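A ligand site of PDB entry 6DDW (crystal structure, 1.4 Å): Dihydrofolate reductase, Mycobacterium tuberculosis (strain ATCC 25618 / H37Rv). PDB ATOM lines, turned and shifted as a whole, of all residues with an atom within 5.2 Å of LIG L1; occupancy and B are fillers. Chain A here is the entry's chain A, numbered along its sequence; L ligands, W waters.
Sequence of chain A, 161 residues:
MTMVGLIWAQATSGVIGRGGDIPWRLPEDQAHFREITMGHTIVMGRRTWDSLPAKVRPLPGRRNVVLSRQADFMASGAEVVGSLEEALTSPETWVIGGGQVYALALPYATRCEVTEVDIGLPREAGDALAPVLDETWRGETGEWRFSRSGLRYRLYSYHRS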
ATOM      1  N   ILE A   7      26.985  -4.616  22.699  1.00  0.00           N
ATOM      2  CA  ILE A   7      27.335  -4.745  24.111  1.00  0.00           C
ATOM      3  C   ILE A   7      26.344  -5.713  24.751  1.00  0.00           C
ATOM      4  O   ILE A   7      25.131  -5.614  24.523  1.00  0.00           O
ATOM      5  CB  ILE A   7      27.323  -3.384  24.832  1.00  0.00           C
ATOM      6  CG1 ILE A   7      27.689  -3.560  26.307  1.00  0.00           C
ATOM      7  CG2 ILE A   7      25.977  -2.678  24.659  1.00  0.00           C
ATOM      8  CD1 ILE A   7      28.036  -2.253  26.984  1.00  0.00           C
ATOM      9  N   TRP A   8      26.857  -6.678  25.526  1.00  0.00           N
ATOM     10  CA  TRP A   8      26.002  -7.606  26.260  1.00  0.00           C
ATOM     11  C   TRP A   8      26.723  -8.192  27.453  1.00  0.00           C
ATOM     12  O   TRP A   8      27.942  -8.105  27.538  1.00  0.00           O
ATOM     13  CB  TRP A   8      25.485  -8.738  25.353  1.00  0.00           C
ATOM     14  CG  TRP A   8      26.493  -9.820  24.977  1.00  0.00           C
ATOM     15  CD1 TRP A   8      26.804 -10.951  25.700  1.00  0.00           C
ATOM     16  CD2 TRP A   8      27.254  -9.898  23.770  1.00  0.00           C
ATOM     17  NE1 TRP A   8      27.745 -11.700  25.032  1.00  0.00           N
ATOM     18  CE2 TRP A   8      28.017 -11.099  23.834  1.00  0.00           C
ATOM     19  CE3 TRP A   8      27.378  -9.084  22.646  1.00  0.00           C
ATOM     20  CZ2 TRP A   8      28.896 -11.479  22.817  1.00  0.00           C
ATOM     21  CZ3 TRP A   8      28.248  -9.474  21.629  1.00  0.00           C
ATOM     22  CH2 TRP A   8      28.983 -10.678  21.726  1.00  0.00           C
ATOM     23  N   ALA A   9      25.946  -8.833  28.333  1.00  0.00           N
ATOM     24  CA  ALA A   9      26.472  -9.632  29.427  1.00  0.00           C
ATOM     25  C   ALA A   9      25.906 -11.035  29.271  1.00  0.00           C
ATOM     26  O   ALA A   9      24.691 -11.213  29.095  1.00  0.00           O
ATOM     27  CB  ALA A   9      26.045  -9.022  30.766  1.00  0.00           C
ATOM     28  N   ILE A  22      16.820 -10.735  32.474  1.00  0.00           N
ATOM     29  CA  ILE A  22      18.198 -11.164  32.593  1.00  0.00           C
ATOM     30  C   ILE A  22      18.308 -11.936  33.895  1.00  0.00           C
ATOM     31  O   ILE A  22      18.001 -11.407  34.953  1.00  0.00           O
ATOM     32  CB  ILE A  22      19.145  -9.952  32.588  1.00  0.00           C
ATOM     33  CG1 ILE A  22      19.072  -9.254  31.226  1.00  0.00           C
ATOM     34  CG2 ILE A  22      20.568 -10.390  32.884  1.00  0.00           C
ATOM     35  CD1 ILE A  22      19.918  -7.989  31.093  1.00  0.00           C
ATOM     36  N   PRO A  27      25.089  -5.235  39.324  1.00  0.00           N
ATOM     37  CA  PRO A  27      24.973  -3.777  39.236  1.00  0.00           C
ATOM     38  C   PRO A  27      26.193  -3.095  38.639  1.00  0.00           C
ATOM     39  O   PRO A  27      26.045  -2.103  37.919  1.00  0.00           O
ATOM     40  CB  PRO A  27      24.799  -3.361  40.696  1.00  0.00           C
ATOM     41  CG  PRO A  27      24.192  -4.510  41.347  1.00  0.00           C
ATOM     42  CD  PRO A  27      24.778  -5.733  40.677  1.00  0.00           C
ATOM     43  N   ASP A  29      28.108  -4.170  36.357  1.00  0.00           N
ATOM     44  CA  ASP A  29      28.100  -4.339  34.927  1.00  0.00           C
ATOM     45  C   ASP A  29      27.125  -3.358  34.271  1.00  0.00           C
ATOM     46  O   ASP A  29      27.396  -2.828  33.187  1.00  0.00           O
ATOM     47  CB  ASP A  29      27.741  -5.782  34.580  1.00  0.00           C
ATOM     48  CG  ASP A  29      27.481  -5.978  33.117  1.00  0.00           C
ATOM     49  OD1 ASP A  29      28.377  -5.696  32.300  1.00  0.00           O
ATOM     50  OD2 ASP A  29      26.358  -6.382  32.798  1.00  0.00           O
ATOM     51  N   GLN A  30      25.999  -3.111  34.930  1.00  0.00           N
ATOM     52  CA  GLN A  30      25.035  -2.146  34.422  1.00  0.00           C
ATOM     53  C   GLN A  30      25.626  -0.742  34.384  1.00  0.00           C
ATOM     54  O   GLN A  30      25.287   0.064  33.508  1.00  0.00           O
ATOM     55  CB  GLN A  30      23.745  -2.141  35.260  1.00  0.00           C
ATOM     56  CG  GLN A  30      22.934  -3.425  35.196  1.00  0.00           C
ATOM     57  CD  GLN A  30      21.683  -3.330  36.041  1.00  0.00           C
ATOM     58  OE1 GLN A  30      21.754  -3.118  37.258  1.00  0.00           O
ATOM     59  NE2 GLN A  30      20.523  -3.468  35.400  1.00  0.00           N
ATOM     60  N   ALA A  31      26.497  -0.417  35.339  1.00  0.00           N
ATOM     61  CA  ALA A  31      27.152   0.883  35.336  1.00  0.00           C
ATOM     62  C   ALA A  31      28.124   0.983  34.161  1.00  0.00           C
ATOM     63  O   ALA A  31      28.241   2.019  33.506  1.00  0.00           O
ATOM     64  CB  ALA A  31      27.854   1.135  36.680  1.00  0.00           C
ATOM     65  N   HIS A  32      28.820  -0.122  33.898  1.00  0.00           N
ATOM     66  CA  HIS A  32      29.685  -0.274  32.725  1.00  0.00           C
ATOM     67  C   HIS A  32      28.891  -0.080  31.436  1.00  0.00           C
ATOM     68  O   HIS A  32      29.324   0.622  30.529  1.00  0.00           O
ATOM     69  CB  HIS A  32      30.309  -1.675  32.779  1.00  0.00           C
ATOM     70  CG  HIS A  32      30.887  -2.158  31.482  1.00  0.00           C
ATOM     71  ND1 HIS A  32      32.011  -1.600  30.919  1.00  0.00           N
ATOM     72  CD2 HIS A  32      30.537  -3.189  30.673  1.00  0.00           C
ATOM     73  CE1 HIS A  32      32.315  -2.244  29.808  1.00  0.00           C
ATOM     74  NE2 HIS A  32      31.442  -3.216  29.642  1.00  0.00           N
ATOM     75  N   PHE A  33      27.711  -0.673  31.384  1.00  0.00           N
ATOM     76  CA  PHE A  33      26.838  -0.522  30.218  1.00  0.00           C
ATOM     77  C   PHE A  33      26.510   0.950  29.977  1.00  0.00           C
ATOM     78  O   PHE A  33      26.586   1.445  28.833  1.00  0.00           O
ATOM     79  CB  PHE A  33      25.569  -1.343  30.411  1.00  0.00           C
ATOM     80  CG  PHE A  33      24.466  -1.031  29.421  1.00  0.00           C
ATOM     81  CD1 PHE A  33      24.335  -1.761  28.244  1.00  0.00           C
ATOM     82  CD2 PHE A  33      23.551  -0.018  29.691  1.00  0.00           C
ATOM     83  CE1 PHE A  33      23.329  -1.458  27.346  1.00  0.00           C
ATOM     84  CE2 PHE A  33      22.545   0.275  28.792  1.00  0.00           C
ATOM     85  CZ  PHE A  33      22.435  -0.446  27.624  1.00  0.00           C
ATOM     86  N   ARG A  34      26.161   1.659  31.048  1.00  0.00           N
ATOM     87  CA  ARG A  34      25.824   3.067  30.941  1.00  0.00           C
ATOM     88  C   ARG A  34      27.009   3.890  30.442  1.00  0.00           C
ATOM     89  O   ARG A  34      26.862   4.756  29.578  1.00  0.00           O
ATOM     90  CB  ARG A  34      25.330   3.593  32.297  1.00  0.00           C
ATOM     91  CG  ARG A  34      25.050   5.081  32.296  1.00  0.00           C
ATOM     92  CD  ARG A  34      24.402   5.532  33.595  1.00  0.00           C
ATOM     93  NE  ARG A  34      25.167   5.082  34.738  1.00  0.00           N
ATOM     94  CZ  ARG A  34      24.712   5.066  35.992  1.00  0.00           C
ATOM     95  NH1 ARG A  34      23.484   5.484  36.264  1.00  0.00           N
ATOM     96  NH2 ARG A  34      25.495   4.634  36.964  1.00  0.00           N
ATOM     97  N   THR A  37      27.576   3.295  26.623  1.00  0.00           N
ATOM     98  CA  THR A  37      26.500   3.717  25.733  1.00  0.00           C
ATOM     99  C   THR A  37      26.106   5.184  25.819  1.00  0.00           C
ATOM    100  O   THR A  37      25.535   5.727  24.862  1.00  0.00           O
ATOM    101  CB  THR A  37      25.230   2.857  25.912  1.00  0.00           C
ATOM    102  OG1 THR A  37      24.762   2.942  27.269  1.00  0.00           O
ATOM    103  CG2 THR A  37      25.502   1.398  25.554  1.00  0.00           C
ATOM    104  N   MET A  38      26.416   5.839  26.954  1.00  0.00           N
ATOM    105  CA  MET A  38      25.984   7.211  27.174  1.00  0.00           C
ATOM    106  C   MET A  38      26.345   8.160  26.027  1.00  0.00           C
ATOM    107  O   MET A  38      27.469   8.141  25.503  1.00  0.00           O
ATOM    108  CB  MET A  38      26.549   7.748  28.479  1.00  0.00           C
ATOM    109  CG  MET A  38      26.026   9.148  28.820  1.00  0.00           C
ATOM    110  SD  MET A  38      24.245   9.179  29.013  1.00  0.00           S
ATOM    111  CE  MET A  38      24.004   7.910  30.248  1.00  0.00           C
ATOM    112  N   THR A  48      13.478  -6.358  24.033  1.00  0.00           N
ATOM    113  CA  THR A  48      14.443  -5.747  24.940  1.00  0.00           C
ATOM    114  C   THR A  48      13.941  -4.393  25.426  1.00  0.00           C
ATOM    115  O   THR A  48      14.077  -4.065  26.601  1.00  0.00           O
ATOM    116  CB  THR A  48      15.848  -5.683  24.313  1.00  0.00           C
ATOM    117  OG1 THR A  48      16.360  -7.019  24.221  1.00  0.00           O
ATOM    118  CG2 THR A  48      16.805  -4.864  25.153  1.00  0.00           C
ATOM    119  N   SER A  51      11.627  -4.991  28.106  1.00  0.00           N
ATOM    120  CA  SER A  51      12.268  -5.491  29.324  1.00  0.00           C
ATOM    121  C   SER A  51      12.892  -4.383  30.180  1.00  0.00           C
ATOM    122  O   SER A  51      13.254  -4.614  31.327  1.00  0.00           O
ATOM    123  CB  SER A  51      13.328  -6.534  28.968  1.00  0.00           C
ATOM    124  OG  SER A  51      14.507  -5.924  28.487  1.00  0.00           O
ATOM    125  N   LEU A  52      13.054  -3.186  29.619  1.00  0.00           N
ATOM    126  CA  LEU A  52      13.651  -2.088  30.385  1.00  0.00           C
ATOM    127  C   LEU A  52      12.696  -1.657  31.484  1.00  0.00           C
ATOM    128  O   LEU A  52      11.492  -1.515  31.240  1.00  0.00           O
ATOM    129  CB  LEU A  52      13.957  -0.904  29.479  1.00  0.00           C
ATOM    130  CG  LEU A  52      14.934  -1.117  28.320  1.00  0.00           C
ATOM    131  CD1 LEU A  52      15.004   0.139  27.480  1.00  0.00           C
ATOM    132  CD2 LEU A  52      16.305  -1.492  28.869  1.00  0.00           C
ATOM    133  N   PRO A  53      13.228  -1.432  32.697  1.00  0.00           N
ATOM    134  CA  PRO A  53      12.390  -0.867  33.771  1.00  0.00           C
ATOM    135  C   PRO A  53      11.787   0.467  33.314  1.00  0.00           C
ATOM    136  O   PRO A  53      12.468   1.255  32.649  1.00  0.00           O
ATOM    137  CB  PRO A  53      13.397  -0.640  34.896  1.00  0.00           C
ATOM    138  CG  PRO A  53      14.465  -1.637  34.667  1.00  0.00           C
ATOM    139  CD  PRO A  53      14.592  -1.737  33.163  1.00  0.00           C
ATOM    140  N   VAL A  56      13.687   3.735  33.393  1.00  0.00           N
ATOM    141  CA  VAL A  56      14.731   4.017  32.404  1.00  0.00           C
ATOM    142  C   VAL A  56      14.328   3.571  31.006  1.00  0.00           C
ATOM    143  O   VAL A  56      15.148   3.064  30.232  1.00  0.00           O
ATOM    144  CB  VAL A  56      16.052   3.339  32.783  1.00  0.00           C
ATOM    145  CG1 VAL A  56      16.678   4.037  33.989  1.00  0.00           C
ATOM    146  CG2 VAL A  56      15.841   1.861  33.045  1.00  0.00           C
ATOM    147  N   LEU A  59      16.099   4.738  27.875  1.00  0.00           N
ATOM    148  CA  LEU A  59      17.356   4.939  28.595  1.00  0.00           C
ATOM    149  C   LEU A  59      17.823   6.381  28.389  1.00  0.00           C
ATOM    150  O   LEU A  59      17.961   6.864  27.260  1.00  0.00           O
ATOM    151  CB  LEU A  59      18.415   3.949  28.114  1.00  0.00           C
ATOM    152  CG  LEU A  59      18.190   2.508  28.604  1.00  0.00           C
ATOM    153  CD1 LEU A  59      18.897   1.489  27.724  1.00  0.00           C
ATOM    154  CD2 LEU A  59      18.655   2.344  30.063  1.00  0.00           C
ATOM    155  N   PRO A  60      18.039   7.108  29.499  1.00  0.00           N
ATOM    156  CA  PRO A  60      18.312   8.541  29.368  1.00  0.00           C
ATOM    157  C   PRO A  60      19.676   8.873  28.772  1.00  0.00           C
ATOM    158  O   PRO A  60      20.654   8.152  28.972  1.00  0.00           O
ATOM    159  CB  PRO A  60      18.257   9.029  30.826  1.00  0.00           C
ATOM    160  CG  PRO A  60      18.597   7.816  31.649  1.00  0.00           C
ATOM    161  CD  PRO A  60      17.972   6.646  30.897  1.00  0.00           C
ATOM    162  N   ARG A  62      20.527   8.869  25.740  1.00  0.00           N
ATOM    163  CA  ARG A  62      20.818   8.061  24.562  1.00  0.00           C
ATOM    164  C   ARG A  62      19.630   8.138  23.604  1.00  0.00           C
ATOM    165  O   ARG A  62      18.499   8.246  24.046  1.00  0.00           O
ATOM    166  CB  ARG A  62      21.079   6.609  24.982  1.00  0.00           C
ATOM    167  CG  ARG A  62      22.486   6.388  25.504  1.00  0.00           C
ATOM    168  CD  ARG A  62      22.584   5.326  26.604  1.00  0.00           C
ATOM    169  NE  ARG A  62      21.931   5.754  27.840  1.00  0.00           N
ATOM    170  CZ  ARG A  62      21.896   5.041  28.957  1.00  0.00           C
ATOM    171  NH1 ARG A  62      22.476   3.842  29.006  1.00  0.00           N
ATOM    172  NH2 ARG A  62      21.270   5.507  30.034  1.00  0.00           N
ATOM    173  N   ILE A  96      22.115  -3.104  21.708  1.00  0.00           N
ATOM    174  CA  ILE A  96      21.995  -3.543  23.082  1.00  0.00           C
ATOM    175  C   ILE A  96      21.008  -4.709  23.227  1.00  0.00           C
ATOM    176  O   ILE A  96      20.452  -4.938  24.305  1.00  0.00           O
ATOM    177  CB  ILE A  96      21.589  -2.365  23.996  1.00  0.00           C
ATOM    178  CG1 ILE A  96      20.159  -1.911  23.732  1.00  0.00           C
ATOM    179  CG2 ILE A  96      22.585  -1.207  23.840  1.00  0.00           C
ATOM    180  CD1 ILE A  96      19.510  -1.228  24.935  1.00  0.00           C
ATOM    181  N   TYR A 102      21.006  -9.040  18.297  1.00  0.00           N
ATOM    182  CA  TYR A 102      22.459  -9.250  18.252  1.00  0.00           C
ATOM    183  C   TYR A 102      22.837 -10.072  17.025  1.00  0.00           C
ATOM    184  O   TYR A 102      23.836  -9.777  16.374  1.00  0.00           O
ATOM    185  CB  TYR A 102      22.976  -9.955  19.508  1.00  0.00           C
ATOM    186  CG  TYR A 102      22.974  -9.147  20.795  1.00  0.00           C
ATOM    187  CD1 TYR A 102      23.485  -7.856  20.872  1.00  0.00           C
ATOM    188  CD2 TYR A 102      22.469  -9.717  21.964  1.00  0.00           C
ATOM    189  CE1 TYR A 102      23.497  -7.147  22.056  1.00  0.00           C
ATOM    190  CE2 TYR A 102      22.471  -9.019  23.148  1.00  0.00           C
ATOM    191  CZ  TYR A 102      22.979  -7.733  23.184  1.00  0.00           C
ATOM    192  OH  TYR A 102      22.961  -7.045  24.369  1.00  0.00           O
ATOM    193  N   GLU A 113      31.592  -5.291  23.286  1.00  0.00           N
ATOM    194  CA  GLU A 113      31.968  -5.117  24.687  1.00  0.00           C
ATOM    195  C   GLU A 113      31.170  -6.142  25.488  1.00  0.00           C
ATOM    196  O   GLU A 113      29.955  -6.020  25.616  1.00  0.00           O
ATOM    197  CB  GLU A 113      31.654  -3.700  25.145  1.00  0.00           C
ATOM    198  CG  GLU A 113      32.546  -2.633  24.524  1.00  0.00           C
ATOM    199  CD  GLU A 113      34.021  -2.757  24.900  1.00  0.00           C
ATOM    200  OE1 GLU A 113      34.302  -3.266  26.004  1.00  0.00           O
ATOM    201  OE2 GLU A 113      34.887  -2.356  24.098  1.00  0.00           O
ATOM    202  N   THR A 115      30.514  -8.761  28.791  1.00  0.00           N
ATOM    203  CA  THR A 115      30.756  -9.140  30.184  1.00  0.00           C
ATOM    204  C   THR A 115      30.466 -10.606  30.343  1.00  0.00           C
ATOM    205  O   THR A 115      29.380 -11.064  29.965  1.00  0.00           O
ATOM    206  CB  THR A 115      29.846  -8.369  31.124  1.00  0.00           C
ATOM    207  OG1 THR A 115      30.096  -6.983  30.959  1.00  0.00           O
ATOM    208  CG2 THR A 115      30.112  -8.765  32.574  1.00  0.00           C
HETATM  209  C1  LIG L   1      23.505  -5.625  30.772  1.00  0.00           C
HETATM  210  C2  LIG L   1      20.896  -4.871  28.403  1.00  0.00           C
HETATM  211  C3  LIG L   1      21.648  -4.644  27.259  1.00  0.00           C
HETATM  212  C4  LIG L   1      19.504  -4.777  28.310  1.00  0.00           C
HETATM  213  N1  LIG L   1      24.957  -5.131  28.472  1.00  0.00           N
HETATM  214  N2  LIG L   1      26.927  -5.509  29.639  1.00  0.00           N
HETATM  215  N3  LIG L   1      24.891  -5.691  30.788  1.00  0.00           N
HETATM  216  O1  LIG L   1      24.306   2.293  36.515  1.00  0.00           O
HETATM  217  C5  LIG L   1      23.294   1.653  36.153  1.00  0.00           C
HETATM  218  O2  LIG L   1      22.636   0.870  36.867  1.00  0.00           O
HETATM  219  C6  LIG L   1      22.799   1.856  34.710  1.00  0.00           C
HETATM  220  C7  LIG L   1      21.277   1.924  34.756  1.00  0.00           C
HETATM  221  C8  LIG L   1      20.647   2.051  33.356  1.00  0.00           C
HETATM  222  C9  LIG L   1      21.404   3.010  32.410  1.00  0.00           C
HETATM  223  O3  LIG L   1      21.284   4.236  32.611  1.00  0.00           O
HETATM  224  O4  LIG L   1      22.040   2.492  31.458  1.00  0.00           O
HETATM  225  N4  LIG L   1      20.470   0.755  32.677  1.00  0.00           N
HETATM  226  C10 LIG L   1      19.513  -0.128  32.991  1.00  0.00           C
HETATM  227  O5  LIG L   1      18.762   0.048  33.956  1.00  0.00           O
HETATM  228  C11 LIG L   1      19.372  -1.245  32.146  1.00  0.00           C
HETATM  229  C12 LIG L   1      18.463  -2.264  32.421  1.00  0.00           C
HETATM  230  C13 LIG L   1      18.302  -3.352  31.582  1.00  0.00           C
HETATM  231  O6  LIG L   1      17.770  -2.131  33.599  1.00  0.00           O
HETATM  232  C14 LIG L   1      20.083  -1.344  30.940  1.00  0.00           C
HETATM  233  C15 LIG L   1      19.930  -2.429  30.080  1.00  0.00           C
HETATM  234  C16 LIG L   1      19.035  -3.463  30.393  1.00  0.00           C
HETATM  235  N5  LIG L   1      18.848  -4.536  29.607  1.00  0.00           N
HETATM  236  N6  LIG L   1      21.519  -5.201  29.540  1.00  0.00           N
HETATM  237  C17 LIG L   1      22.858  -5.280  29.588  1.00  0.00           C
HETATM  238  O7  LIG L   1      22.876  -5.860  31.815  1.00  0.00           O
HETATM  239  C18 LIG L   1      25.600  -5.451  29.608  1.00  0.00           C
HETATM  240  C19 LIG L   1      23.630  -5.055  28.452  1.00  0.00           C
HETATM  241  N7  LIG L   1      23.036  -4.742  27.291  1.00  0.00           N
HETATM  242  P1  LG2 L   2      14.831  -8.991  20.964  1.00  0.00           P
HETATM  243  O1  LG2 L   2      15.938  -9.300  20.047  1.00  0.00           O
HETATM  244  O2  LG2 L   2      15.058  -8.068  22.123  1.00  0.00           O
HETATM  245  O3  LG2 L   2      13.519  -8.390  20.182  1.00  0.00           O
HETATM  246  C1  LG2 L   2      13.061  -9.269  19.166  1.00  0.00           C
HETATM  247  C2  LG2 L   2      11.973  -8.453  18.450  1.00  0.00           C
HETATM  248  O4  LG2 L   2      12.609  -7.506  17.614  1.00  0.00           O
HETATM  249  C3  LG2 L   2      11.031  -9.286  17.547  1.00  0.00           C
HETATM  250  O5  LG2 L   2       9.973  -9.834  18.298  1.00  0.00           O
HETATM  251  C4  LG2 L   2      10.505  -8.135  16.632  1.00  0.00           C
HETATM  252  O6  LG2 L   2       9.759  -7.219  17.251  1.00  0.00           O
HETATM  253  C5  LG2 L   2      11.842  -7.370  16.397  1.00  0.00           C
HETATM  254  N1  LG2 L   2      12.605  -7.861  15.286  1.00  0.00           N
HETATM  255  C6  LG2 L   2      13.426  -8.996  15.212  1.00  0.00           C
HETATM  256  N2  LG2 L   2      13.999  -9.167  14.019  1.00  0.00           N
HETATM  257  C7  LG2 L   2      13.506  -8.083  13.266  1.00  0.00           C
HETATM  258  C8  LG2 L   2      13.720  -7.689  11.939  1.00  0.00           C
HETATM  259  N3  LG2 L   2      14.549  -8.422  11.111  1.00  0.00           N
HETATM  260  N4  LG2 L   2      13.117  -6.564  11.451  1.00  0.00           N
HETATM  261  C9  LG2 L   2      12.302  -5.886  12.323  1.00  0.00           C
HETATM  262  N5  LG2 L   2      12.003  -6.136  13.611  1.00  0.00           N
HETATM  263  C10 LG2 L   2      12.634  -7.267  14.056  1.00  0.00           C
HETATM  264  O7  LG2 L   2      14.110 -10.413  21.534  1.00  0.00           O
HETATM  265  P2  LG2 L   2      14.898 -11.684  22.174  1.00  0.00           P
HETATM  266  O8  LG2 L   2      13.789 -12.475  22.752  1.00  0.00           O
HETATM  267  O9  LG2 L   2      15.927 -12.274  21.244  1.00  0.00           O
HETATM  268  O10 LG2 L   2      15.869 -11.080  23.434  1.00  0.00           O
HETATM  269  C11 LG2 L   2      15.158 -10.631  24.566  1.00  0.00           C
HETATM  270  C12 LG2 L   2      15.861 -11.232  25.789  1.00  0.00           C
HETATM  271  O11 LG2 L   2      17.245 -10.829  25.844  1.00  0.00           O
HETATM  272  C13 LG2 L   2      15.205 -10.773  27.119  1.00  0.00           C
HETATM  273  O12 LG2 L   2      15.216 -11.882  27.989  1.00  0.00           O
HETATM  274  C14 LG2 L   2      16.172  -9.685  27.614  1.00  0.00           C
HETATM  275  O13 LG2 L   2      16.187  -9.523  29.012  1.00  0.00           O
HETATM  276  C15 LG2 L   2      17.510 -10.315  27.160  1.00  0.00           C
HETATM  277  N6  LG2 L   2      18.590  -9.329  27.019  1.00  0.00           N
HETATM  278  C16 LG2 L   2      19.777  -9.555  27.679  1.00  0.00           C
HETATM  279  C17 LG2 L   2      20.845  -8.746  27.490  1.00  0.00           C
HETATM  280  C18 LG2 L   2      22.084  -9.014  28.171  1.00  0.00           C
HETATM  281  O14 LG2 L   2      23.130  -8.379  27.915  1.00  0.00           O
HETATM  282  N7  LG2 L   2      22.121  -9.993  29.144  1.00  0.00           N
HETATM  283  C19 LG2 L   2      20.801  -7.594  26.587  1.00  0.00           C
HETATM  284  C20 LG2 L   2      19.475  -7.419  25.933  1.00  0.00           C
HETATM  285  C21 LG2 L   2      18.449  -8.231  26.148  1.00  0.00           C
HETATM  286  P3  LG2 L   2       7.970  -7.357  17.054  1.00  0.00           P
HETATM  287  O15 LG2 L   2       7.787  -8.685  17.713  1.00  0.00           O
HETATM  288  O16 LG2 L   2       7.441  -6.142  17.809  1.00  0.00           O
HETATM  289  O17 LG2 L   2       7.845  -7.329  15.564  1.00  0.00           O
HETATM  290  O   HOH W   1      29.762  -5.490  28.552  1.00  0.00           O
HETATM  291  O   HOH W   2      24.763   0.011  38.688  1.00  0.00           O
HETATM  292  O   HOH W   3      17.706   0.837  36.402  1.00  0.00           O
HETATM  293  O   HOH W   4      24.095  -7.647  33.809  1.00  0.00           O
HETATM  294  O   HOH W   5      16.823  -6.926  29.491  1.00  0.00           O
HETATM  295  O   HOH W   6      20.530   5.745  34.545  1.00  0.00           O
HETATM  296  O   HOH W   7      20.704  -4.862  32.827  1.00  0.00           O
HETATM  297  O   HOH W   8      16.944  -4.451  35.131  1.00  0.00           O
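N3 of LIG L1 sits at hydrogen-bond distance from OD2 of Asp 29, at 2.6 Å. An oxygen (O1) of LIG L1 is in salt-bridge range of the guanidinium group (NH2) of Arg 34, 2.7 Å away. O4 of LIG L1 lies within salt-bridge range of NH1 of Arg 62, at 2.8 Å. The backbone carbonyl oxygen (O) of Trp 8 sits close to a nitrogen (N2) of LIG L1, at 3.5 Å. N of Ala 9 lies within hydrogen-bond range of O14 of LG2 L2. The backbone carbonyl oxygen (O) of Ala 9 is in hydrogen-bond range of a nitrogen (N7) of LG2 L2, at 2.8 Å. N of Thr 48 is in hydrogen-bond range of O2 of LG2 L2. OG1 of Thr 48 sits at hydrogen-bond distance from O2 of LG2 L2 (2.7 Å).
OD1 of Asp 29 sits at hydrogen-bond distance from OG1 of Thr 115. The guanidinium group (NH2) of Arg 62 lies within hydrogen-bond range of the backbone carbonyl oxygen (O) of Pro 60, 2.9 Å away. The guanidinium group of Arg 62 is in hydrogen-bond range of the side-chain hydroxyl of Thr 37 (3.0 Å). O of Ile 96 lies close to OH of Tyr 102 (3.3 Å). The side-chain hydroxyl (OG1) of Thr 37 lies within hydrogen-bond range of the backbone carbonyl oxygen (O) of Phe 33 (2.8 Å). O of Trp 8 is in hydrogen-bond range of N of Thr 115 (2.9 Å). N of Trp 8 lies within hydrogen-bond range of O of Glu 113 (3.2 Å). The backbone carbonyl oxygen (O) of Ile 7 lies within hydrogen-bond range of the side-chain hydroxyl (OH) of Tyr 102 (2.6 Å).
Residues that only touch LIG L1: Ile 7, Ala 9, Ile 22, Gln 30, Ala 31, Phe 33, Leu 52, Pro 53, Val 56, Leu 59, Ile 96, Tyr 102 and Thr 115. Hydrophobic or aromatic side chains that line LIG L1: Ile 7, Ala 9, Ile 22, Ala 31, Phe 33, Leu 52, Pro 53, Val 56, Leu 59 and Ile 96. 17 residues have an atom within 4 Å of LIG L1: Ile 7, Trp 8, Ala 9, Ile 22, Asp 29, Gln 30, Ala 31, Phe 33, Arg 34, Leu 52, Pro 53, Val 56, Leu 59, Arg 62, Ile 96, Tyr 102 and Thr 115. Along chain A the residues within 4 Å of LIG L1 span positions 7 to 115. The nearest printed residue that does not touch LIG L1 is Thr 48 (4.2 Å).
Water W6 bridges an oxygen (O3) of LIG L1 (2.6 Å) and the guanidinium group (NH1) of Arg 34 (3.4 Å). Water W7 lies within hydrogen-bond range of O7 of LIG L1 (2.6 Å) and NE2 of Gln 30 (2.9 Å). Water W2 lies within hydrogen-bond range of the backbone carbonyl oxygen of Pro 27 and an oxygen (O2) of LIG L1. Water W4 bridges OD2 of Asp 29 (2.8 Å) and O7 of LIG L1 (2.9 Å). Water W1 lies within hydrogen-bond range of the side-chain hydroxyl of Thr 115 (2.9 Å), the backbone carbonyl oxygen of Glu 113 (3.0 Å), a ring nitrogen (NE2) of His 32 (3.0 Å), a nitrogen (N2) of LIG L1 (3.0 Å) and the backbone carbonyl oxygen of Trp 8 (3.3 Å). Water W5 lies within hydrogen-bond range of an oxygen (O13) of LG2 L2 (2.7 Å), the side-chain hydroxyl of Ser 51 (2.7 Å) and a nitrogen (N5) of LIG L1 (3.1 Å).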
